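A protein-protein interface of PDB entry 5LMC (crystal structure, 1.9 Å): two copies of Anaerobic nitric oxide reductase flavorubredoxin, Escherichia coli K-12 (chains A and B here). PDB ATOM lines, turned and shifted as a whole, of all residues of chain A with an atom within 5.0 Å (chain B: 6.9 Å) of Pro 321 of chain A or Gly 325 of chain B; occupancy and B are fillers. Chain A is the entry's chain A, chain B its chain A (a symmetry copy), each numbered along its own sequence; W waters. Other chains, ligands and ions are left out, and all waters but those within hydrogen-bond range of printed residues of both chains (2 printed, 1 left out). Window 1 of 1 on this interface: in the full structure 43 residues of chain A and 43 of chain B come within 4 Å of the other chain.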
ATOM      1  N   MET A 315      21.063  23.541 -16.133  1.00  0.00           N
ATOM      2  CA  MET A 315      21.861  22.347 -15.884  1.00  0.00           C
ATOM      3  C   MET A 315      20.948  21.118 -15.882  1.00  0.00           C
ATOM      4  O   MET A 315      20.113  20.965 -14.985  1.00  0.00           O
ATOM      5  CB  MET A 315      22.553  22.479 -14.524  1.00  0.00           C
ATOM      6  CG  MET A 315      23.377  21.249 -14.084  1.00  0.00           C
ATOM      7  SD  MET A 315      23.921  21.426 -12.348  1.00  0.00           S
ATOM      8  CE  MET A 315      24.738  19.856 -12.067  1.00  0.00           C
ATOM      9  N   MET A 319      17.289  24.126 -12.742  1.00  0.00           N
ATOM     10  CA  MET A 319      18.089  25.229 -12.179  1.00  0.00           C
ATOM     11  C   MET A 319      19.332  24.646 -11.542  1.00  0.00           C
ATOM     12  O   MET A 319      19.350  23.471 -11.195  1.00  0.00           O
ATOM     13  CB  MET A 319      17.332  25.905 -11.029  1.00  0.00           C
ATOM     14  CG  MET A 319      16.410  27.045 -11.356  1.00  0.00           C
ATOM     15  SD  MET A 319      15.615  27.502  -9.796  1.00  0.00           S
ATOM     16  CE  MET A 319      14.210  26.408  -9.851  1.00  0.00           C
ATOM     17  N   MET A 320      20.357  25.468 -11.319  1.00  0.00           N
ATOM     18  CA  MET A 320      21.481  24.992 -10.526  1.00  0.00           C
ATOM     19  C   MET A 320      20.991  24.768  -9.086  1.00  0.00           C
ATOM     20  O   MET A 320      20.223  25.555  -8.564  1.00  0.00           O
ATOM     21  CB  MET A 320      22.660  25.958 -10.610  1.00  0.00           C
ATOM     22  CG  MET A 320      23.423  25.808 -11.935  1.00  0.00           C
ATOM     23  SD  MET A 320      24.922  26.785 -12.019  1.00  0.00           S
ATOM     24  CE  MET A 320      26.000  25.816 -10.949  1.00  0.00           C
ATOM     25  N   PRO A 321      21.410  23.666  -8.463  1.00  0.00           N
ATOM     26  CA  PRO A 321      20.858  23.254  -7.156  1.00  0.00           C
ATOM     27  C   PRO A 321      20.944  24.280  -6.027  1.00  0.00           C
ATOM     28  O   PRO A 321      19.987  24.383  -5.272  1.00  0.00           O
ATOM     29  CB  PRO A 321      21.690  22.017  -6.780  1.00  0.00           C
ATOM     30  CG  PRO A 321      22.848  21.998  -7.729  1.00  0.00           C
ATOM     31  CD  PRO A 321      22.396  22.704  -8.981  1.00  0.00           C
ATOM     32  N   LYS A 322      22.062  24.986  -5.873  1.00  0.00           N
ATOM     33  CA  LYS A 322      22.170  25.943  -4.773  1.00  0.00           C
ATOM     34  C   LYS A 322      21.186  27.097  -4.933  1.00  0.00           C
ATOM     35  O   LYS A 322      20.771  27.701  -3.945  1.00  0.00           O
ATOM     36  CB  LYS A 322      23.586  26.501  -4.657  1.00  0.00           C
ATOM     37  CG  LYS A 322      24.632  25.430  -4.345  1.00  0.00           C
ATOM     38  CD  LYS A 322      25.940  26.078  -3.910  1.00  0.00           C
ATOM     39  CE  LYS A 322      27.091  25.087  -4.011  1.00  0.00           C
ATOM     40  NZ  LYS A 322      27.318  24.710  -5.442  1.00  0.00           N
ATOM     41  N   ILE A 323      20.852  27.432  -6.177  1.00  0.00           N
ATOM     42  CA  ILE A 323      19.834  28.456  -6.431  1.00  0.00           C
ATOM     43  C   ILE A 323      18.442  27.909  -6.103  1.00  0.00           C
ATOM     44  O   ILE A 323      17.626  28.599  -5.491  1.00  0.00           O
ATOM     45  CB  ILE A 323      19.892  28.972  -7.896  1.00  0.00           C
ATOM     46  CG1 ILE A 323      21.235  29.677  -8.146  1.00  0.00           C
ATOM     47  CG2 ILE A 323      18.725  29.921  -8.185  1.00  0.00           C
ATOM     48  CD1 ILE A 323      21.394  30.976  -7.349  1.00  0.00           C
ATOM     49  N   ALA A 324      18.161  26.668  -6.502  1.00  0.00           N
ATOM     50  CA  ALA A 324      16.895  26.060  -6.106  1.00  0.00           C
ATOM     51  C   ALA A 324      16.748  26.044  -4.574  1.00  0.00           C
ATOM     52  O   ALA A 324      15.682  26.372  -4.044  1.00  0.00           O
ATOM     53  CB  ALA A 324      16.729  24.633  -6.708  1.00  0.00           C
ATOM     54  N   GLY A 325      17.809  25.686  -3.855  1.00  0.00           N
ATOM     55  CA  GLY A 325      17.743  25.682  -2.393  1.00  0.00           C
ATOM     56  C   GLY A 325      17.509  27.054  -1.757  1.00  0.00           C
ATOM     57  O   GLY A 325      16.761  27.203  -0.779  1.00  0.00           O
ATOM     58  N   GLU B  26      29.750  21.989  -8.614  1.00  0.00           N
ATOM     59  CA  GLU B  26      28.807  20.863  -8.739  1.00  0.00           C
ATOM     60  C   GLU B  26      29.474  19.485  -8.836  1.00  0.00           C
ATOM     61  O   GLU B  26      28.845  18.472  -8.541  1.00  0.00           O
ATOM     62  CB  GLU B  26      27.854  21.057  -9.920  1.00  0.00           C
ATOM     63  CG  GLU B  26      27.000  22.296  -9.795  1.00  0.00           C
ATOM     64  CD  GLU B  26      26.349  22.398  -8.432  1.00  0.00           C
ATOM     65  OE1 GLU B  26      25.821  21.378  -7.941  1.00  0.00           O
ATOM     66  OE2 GLU B  26      26.363  23.493  -7.841  1.00  0.00           O
ATOM     67  N   LYS B 295      28.607  15.836  -1.614  1.00  0.00           N
ATOM     68  CA  LYS B 295      27.368  15.653  -2.367  1.00  0.00           C
ATOM     69  C   LYS B 295      27.496  14.659  -3.530  1.00  0.00           C
ATOM     70  O   LYS B 295      26.576  13.872  -3.809  1.00  0.00           O
ATOM     71  CB  LYS B 295      26.893  17.020  -2.885  1.00  0.00           C
ATOM     72  CG  LYS B 295      25.600  16.975  -3.661  1.00  0.00           C
ATOM     73  CD  LYS B 295      25.553  18.094  -4.711  1.00  0.00           C
ATOM     74  CE  LYS B 295      26.454  17.762  -5.892  1.00  0.00           C
ATOM     75  NZ  LYS B 295      26.370  18.758  -7.003  1.00  0.00           N
ATOM     76  N   MET B 319      10.824  22.924   3.088  1.00  0.00           N
ATOM     77  CA  MET B 319      11.869  21.903   3.285  1.00  0.00           C
ATOM     78  C   MET B 319      13.151  22.596   3.687  1.00  0.00           C
ATOM     79  O   MET B 319      13.320  23.781   3.417  1.00  0.00           O
ATOM     80  CB  MET B 319      12.192  21.208   1.955  1.00  0.00           C
ATOM     81  CG  MET B 319      11.396  19.992   1.575  1.00  0.00           C
ATOM     82  SD  MET B 319      11.964  19.525  -0.078  1.00  0.00           S
ATOM     83  CE  MET B 319      10.850  20.508  -1.060  1.00  0.00           C
ATOM     84  N   MET B 320      14.095  21.861   4.275  1.00  0.00           N
ATOM     85  CA  MET B 320      15.411  22.444   4.486  1.00  0.00           C
ATOM     86  C   MET B 320      16.061  22.675   3.113  1.00  0.00           C
ATOM     87  O   MET B 320      15.943  21.849   2.226  1.00  0.00           O
ATOM     88  CB  MET B 320      16.259  21.567   5.405  1.00  0.00           C
ATOM     89  CG  MET B 320      15.856  21.732   6.879  1.00  0.00           C
ATOM     90  SD  MET B 320      16.930  20.869   8.021  1.00  0.00           S
ATOM     91  CE  MET B 320      18.372  21.949   7.989  1.00  0.00           C
ATOM     92  N   PRO B 321      16.712  23.825   2.930  1.00  0.00           N
ATOM     93  CA  PRO B 321      17.209  24.234   1.600  1.00  0.00           C
ATOM     94  C   PRO B 321      18.141  23.252   0.890  1.00  0.00           C
ATOM     95  O   PRO B 321      18.002  23.102  -0.316  1.00  0.00           O
ATOM     96  CB  PRO B 321      17.970  25.541   1.879  1.00  0.00           C
ATOM     97  CG  PRO B 321      18.120  25.617   3.367  1.00  0.00           C
ATOM     98  CD  PRO B 321      16.974  24.841   3.962  1.00  0.00           C
ATOM     99  N   LYS B 322      19.094  22.637   1.589  1.00  0.00           N
ATOM    100  CA  LYS B 322      20.014  21.725   0.912  1.00  0.00           C
ATOM    101  C   LYS B 322      19.292  20.496   0.370  1.00  0.00           C
ATOM    102  O   LYS B 322      19.738  19.895  -0.605  1.00  0.00           O
ATOM    103  CB  LYS B 322      21.140  21.279   1.843  1.00  0.00           C
ATOM    104  CG  LYS B 322      22.018  22.434   2.323  1.00  0.00           C
ATOM    105  CD  LYS B 322      23.298  21.900   2.953  1.00  0.00           C
ATOM    106  CE  LYS B 322      23.967  22.971   3.804  1.00  0.00           C
ATOM    107  NZ  LYS B 322      23.093  23.320   4.969  1.00  0.00           N
ATOM    108  N   ILE B 323      18.207  20.100   1.029  1.00  0.00           N
ATOM    109  CA  ILE B 323      17.386  18.995   0.527  1.00  0.00           C
ATOM    110  C   ILE B 323      16.590  19.446  -0.702  1.00  0.00           C
ATOM    111  O   ILE B 323      16.495  18.715  -1.690  1.00  0.00           O
ATOM    112  CB  ILE B 323      16.435  18.440   1.624  1.00  0.00           C
ATOM    113  CG1 ILE B 323      17.262  17.829   2.767  1.00  0.00           C
ATOM    114  CG2 ILE B 323      15.478  17.397   1.038  1.00  0.00           C
ATOM    115  CD1 ILE B 323      18.031  16.571   2.353  1.00  0.00           C
ATOM    116  N   ALA B 324      16.018  20.648  -0.655  1.00  0.00           N
ATOM    117  CA  ALA B 324      15.355  21.173  -1.844  1.00  0.00           C
ATOM    118  C   ALA B 324      16.327  21.224  -3.037  1.00  0.00           C
ATOM    119  O   ALA B 324      15.970  20.834  -4.152  1.00  0.00           O
ATOM    120  CB  ALA B 324      14.708  22.564  -1.578  1.00  0.00           C
ATOM    121  N   GLY B 325      17.556  21.684  -2.813  1.00  0.00           N
ATOM    122  CA  GLY B 325      18.536  21.728  -3.899  1.00  0.00           C
ATOM    123  C   GLY B 325      18.920  20.362  -4.473  1.00  0.00           C
ATOM    124  O   GLY B 325      19.091  20.187  -5.689  1.00  0.00           O
ATOM    125  N   LEU B 326      19.075  19.378  -3.603  1.00  0.00           N
ATOM    126  CA  LEU B 326      19.481  18.047  -4.050  1.00  0.00           C
ATOM    127  C   LEU B 326      18.328  17.363  -4.805  1.00  0.00           C
ATOM    128  O   LEU B 326      18.553  16.601  -5.742  1.00  0.00           O
ATOM    129  CB  LEU B 326      19.938  17.209  -2.852  1.00  0.00           C
ATOM    130  CG  LEU B 326      20.786  15.953  -3.052  1.00  0.00           C
ATOM    131  CD1 LEU B 326      21.868  16.141  -4.109  1.00  0.00           C
ATOM    132  CD2 LEU B 326      21.400  15.569  -1.711  1.00  0.00           C
ATOM    133  N   VAL B 327      17.092  17.644  -4.401  1.00  0.00           N
ATOM    134  CA  VAL B 327      15.941  17.116  -5.141  1.00  0.00           C
ATOM    135  C   VAL B 327      15.834  17.765  -6.529  1.00  0.00           C
ATOM    136  O   VAL B 327      15.523  17.097  -7.509  1.00  0.00           O
ATOM    137  CB  VAL B 327      14.629  17.223  -4.334  1.00  0.00           C
ATOM    138  CG1 VAL B 327      13.457  16.685  -5.144  1.00  0.00           C
ATOM    139  CG2 VAL B 327      14.754  16.411  -3.047  1.00  0.00           C
ATOM    140  N   GLU B 328      16.103  19.061  -6.619  1.00  0.00           N
ATOM    141  CA  GLU B 328      16.150  19.709  -7.925  1.00  0.00           C
ATOM    142  C   GLU B 328      17.205  19.009  -8.781  1.00  0.00           C
ATOM    143  O   GLU B 328      16.948  18.641  -9.933  1.00  0.00           O
ATOM    144  CB  GLU B 328      16.488  21.198  -7.782  1.00  0.00           C
ATOM    145  CG  GLU B 328      16.640  21.950  -9.117  1.00  0.00           C
ATOM    146  CD  GLU B 328      15.326  22.436  -9.693  1.00  0.00           C
ATOM    147  OE1 GLU B 328      14.247  22.004  -9.213  1.00  0.00           O
ATOM    148  OE2 GLU B 328      15.363  23.252 -10.646  1.00  0.00           O
ATOM    149  N   GLU B 329      18.398  18.838  -8.222  1.00  0.00           N
ATOM    150  CA  GLU B 329      19.479  18.200  -8.962  1.00  0.00           C
ATOM    151  C   GLU B 329      19.130  16.785  -9.406  1.00  0.00           C
ATOM    152  O   GLU B 329      19.401  16.422 -10.551  1.00  0.00           O
ATOM    153  CB  GLU B 329      20.804  18.205  -8.193  1.00  0.00           C
ATOM    154  CG  GLU B 329      21.918  17.568  -9.021  1.00  0.00           C
ATOM    155  CD  GLU B 329      23.304  17.776  -8.448  1.00  0.00           C
ATOM    156  OE1 GLU B 329      23.434  18.257  -7.303  1.00  0.00           O
ATOM    157  OE2 GLU B 329      24.271  17.451  -9.168  1.00  0.00           O
ATOM    158  N   MET B 330      18.546  15.988  -8.507  1.00  0.00           N
ATOM    159  CA  MET B 330      18.111  14.630  -8.865  1.00  0.00           C
ATOM    160  C   MET B 330      17.053  14.610  -9.969  1.00  0.00           C
ATOM    161  O   MET B 330      17.045  13.712 -10.811  1.00  0.00           O
ATOM    162  CB  MET B 330      17.596  13.873  -7.634  1.00  0.00           C
ATOM    163  CG  MET B 330      18.699  13.553  -6.642  1.00  0.00           C
ATOM    164  SD  MET B 330      18.106  12.411  -5.381  1.00  0.00           S
ATOM    165  CE  MET B 330      17.062  13.503  -4.447  1.00  0.00           C
ATOM    166  N   ARG B 359       7.860  15.859  -4.526  1.00  0.00           N
ATOM    167  CA  ARG B 359       8.957  16.200  -5.435  1.00  0.00           C
ATOM    168  C   ARG B 359       9.788  14.979  -5.824  1.00  0.00           C
ATOM    169  O   ARG B 359      10.280  14.890  -6.950  1.00  0.00           O
ATOM    170  CB  ARG B 359       9.847  17.299  -4.838  1.00  0.00           C
ATOM    171  CG  ARG B 359       9.103  18.639  -4.739  1.00  0.00           C
ATOM    172  CD  ARG B 359      10.012  19.783  -4.305  1.00  0.00           C
ATOM    173  NE  ARG B 359       9.239  20.998  -4.048  1.00  0.00           N
ATOM    174  CZ  ARG B 359       9.762  22.181  -3.730  1.00  0.00           C
ATOM    175  NH1 ARG B 359      11.080  22.340  -3.629  1.00  0.00           N
ATOM    176  NH2 ARG B 359       8.959  23.212  -3.512  1.00  0.00           N
HETATM  177  O   HOH W   1      24.315  25.047  -7.671  1.00  0.00           O
HETATM  178  O   HOH W   2      28.300  25.425  -8.214  1.00  0.00           O
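The side-chain carboxylate of Glu 329 of chain B is in salt-bridge range of the side-chain amino group of Lys 295 of chain B (3.0 Å). The side-chain carboxylate of Glu 26 of chain B lies within salt-bridge range of the side-chain amino group of Lys 295 of chain B (2.8 Å).
Printed residues of chain B that touch a printed residue of chain A: Glu 26, Pro 321, Gly 325, Glu 328 and Glu 329. Of the 8 printed residues of chain A, 7 touch a printed residue of chain B. Printed residues of chain A that touch a printed residue of chain B: Met 315, Met 319, Met 320, Pro 321, Lys 322, Ala 324 and Gly 325. Among the printed residues, 10 pairs touch across the chains. Among the printed residues, Asp or Glu carboxylates within 4 Å of a Lys or Arg side-chain nitrogen of the other chain: Lys 322 of chain A with Glu 26 of chain B.
Water W1 lies within hydrogen-bond range of the side-chain carboxylate (OE2) of Glu 26 of chain B (2.6 Å) and the backbone NH (N) of Lys 322 of chain A (2.9 Å). Water W2 lies within hydrogen-bond range of OE2 of Glu 26 of chain B and NZ of Lys 322 of chain A.
Pro 321 of chain A touches Gly 325 of chain B, and with the chains exchanged Gly 325 of chain A touches Pro 321 of chain B. Of the 10 pairs that touch across the chains among the printed residues, 2 have their exchanged pair printed and touching as well.
Among the printed residues, merely in contact across the chains: Pro 321 of chain A with Glu 26 of chain B (3.0 Å), Gly 325 of chain A with Pro 321 of chain B (3.3 Å), Pro 321 of chain A with Gly 325 of chain B (3.3 Å), Ala 324 of chain A with Glu 328 of chain B (3.6 Å), Met 315 of chain A with Glu 329 of chain B (3.8 Å), Pro 321 of chain A with Glu 329 of chain B (3.8 Å), Met 320 of chain A with Glu 26 of chain B (3.8 Å) and Met 315 of chain A with Glu 26 of chain B (3.97 Å).
The side-chain carboxylate (OE2) of Glu 26 of chain B lies within salt-bridge range of the side-chain amino group (NZ) of Lys 322 of chain A (2.9 Å). N of Met 319 of chain A lies within hydrogen-bond range of OE2 of Glu 328 of chain B.
Of the printed residues of chain B, Met 315 of chain A touches Glu 26 (3.97 Å) and Glu 329 (3.8 Å). Of the printed residues of chain B, Met 320 of chain A touches Glu 26. Pro 321 of chain A touches just these residues of chain B: Glu 26, Gly 325 and Glu 329. Of the printed residues of chain B, Ala 324 of chain A touches Glu 328 (3.6 Å). Gly 325 of chain B touches one residue of chain A. Of the printed residues of chain A, Glu 329 of chain B touches Met 315 (3.8 Å) and Pro 321 (3.8 Å). Arg 359 of chain B touches none of the printed residues of chain A. The nearest residue of chain A that does not touch Gly 325 of chain B is Gly 325 of chain A (4.02 Å). The nearest printed residue of chain A that does not touch Glu 329 of chain B is Met 319 of chain A (5.6 Å).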
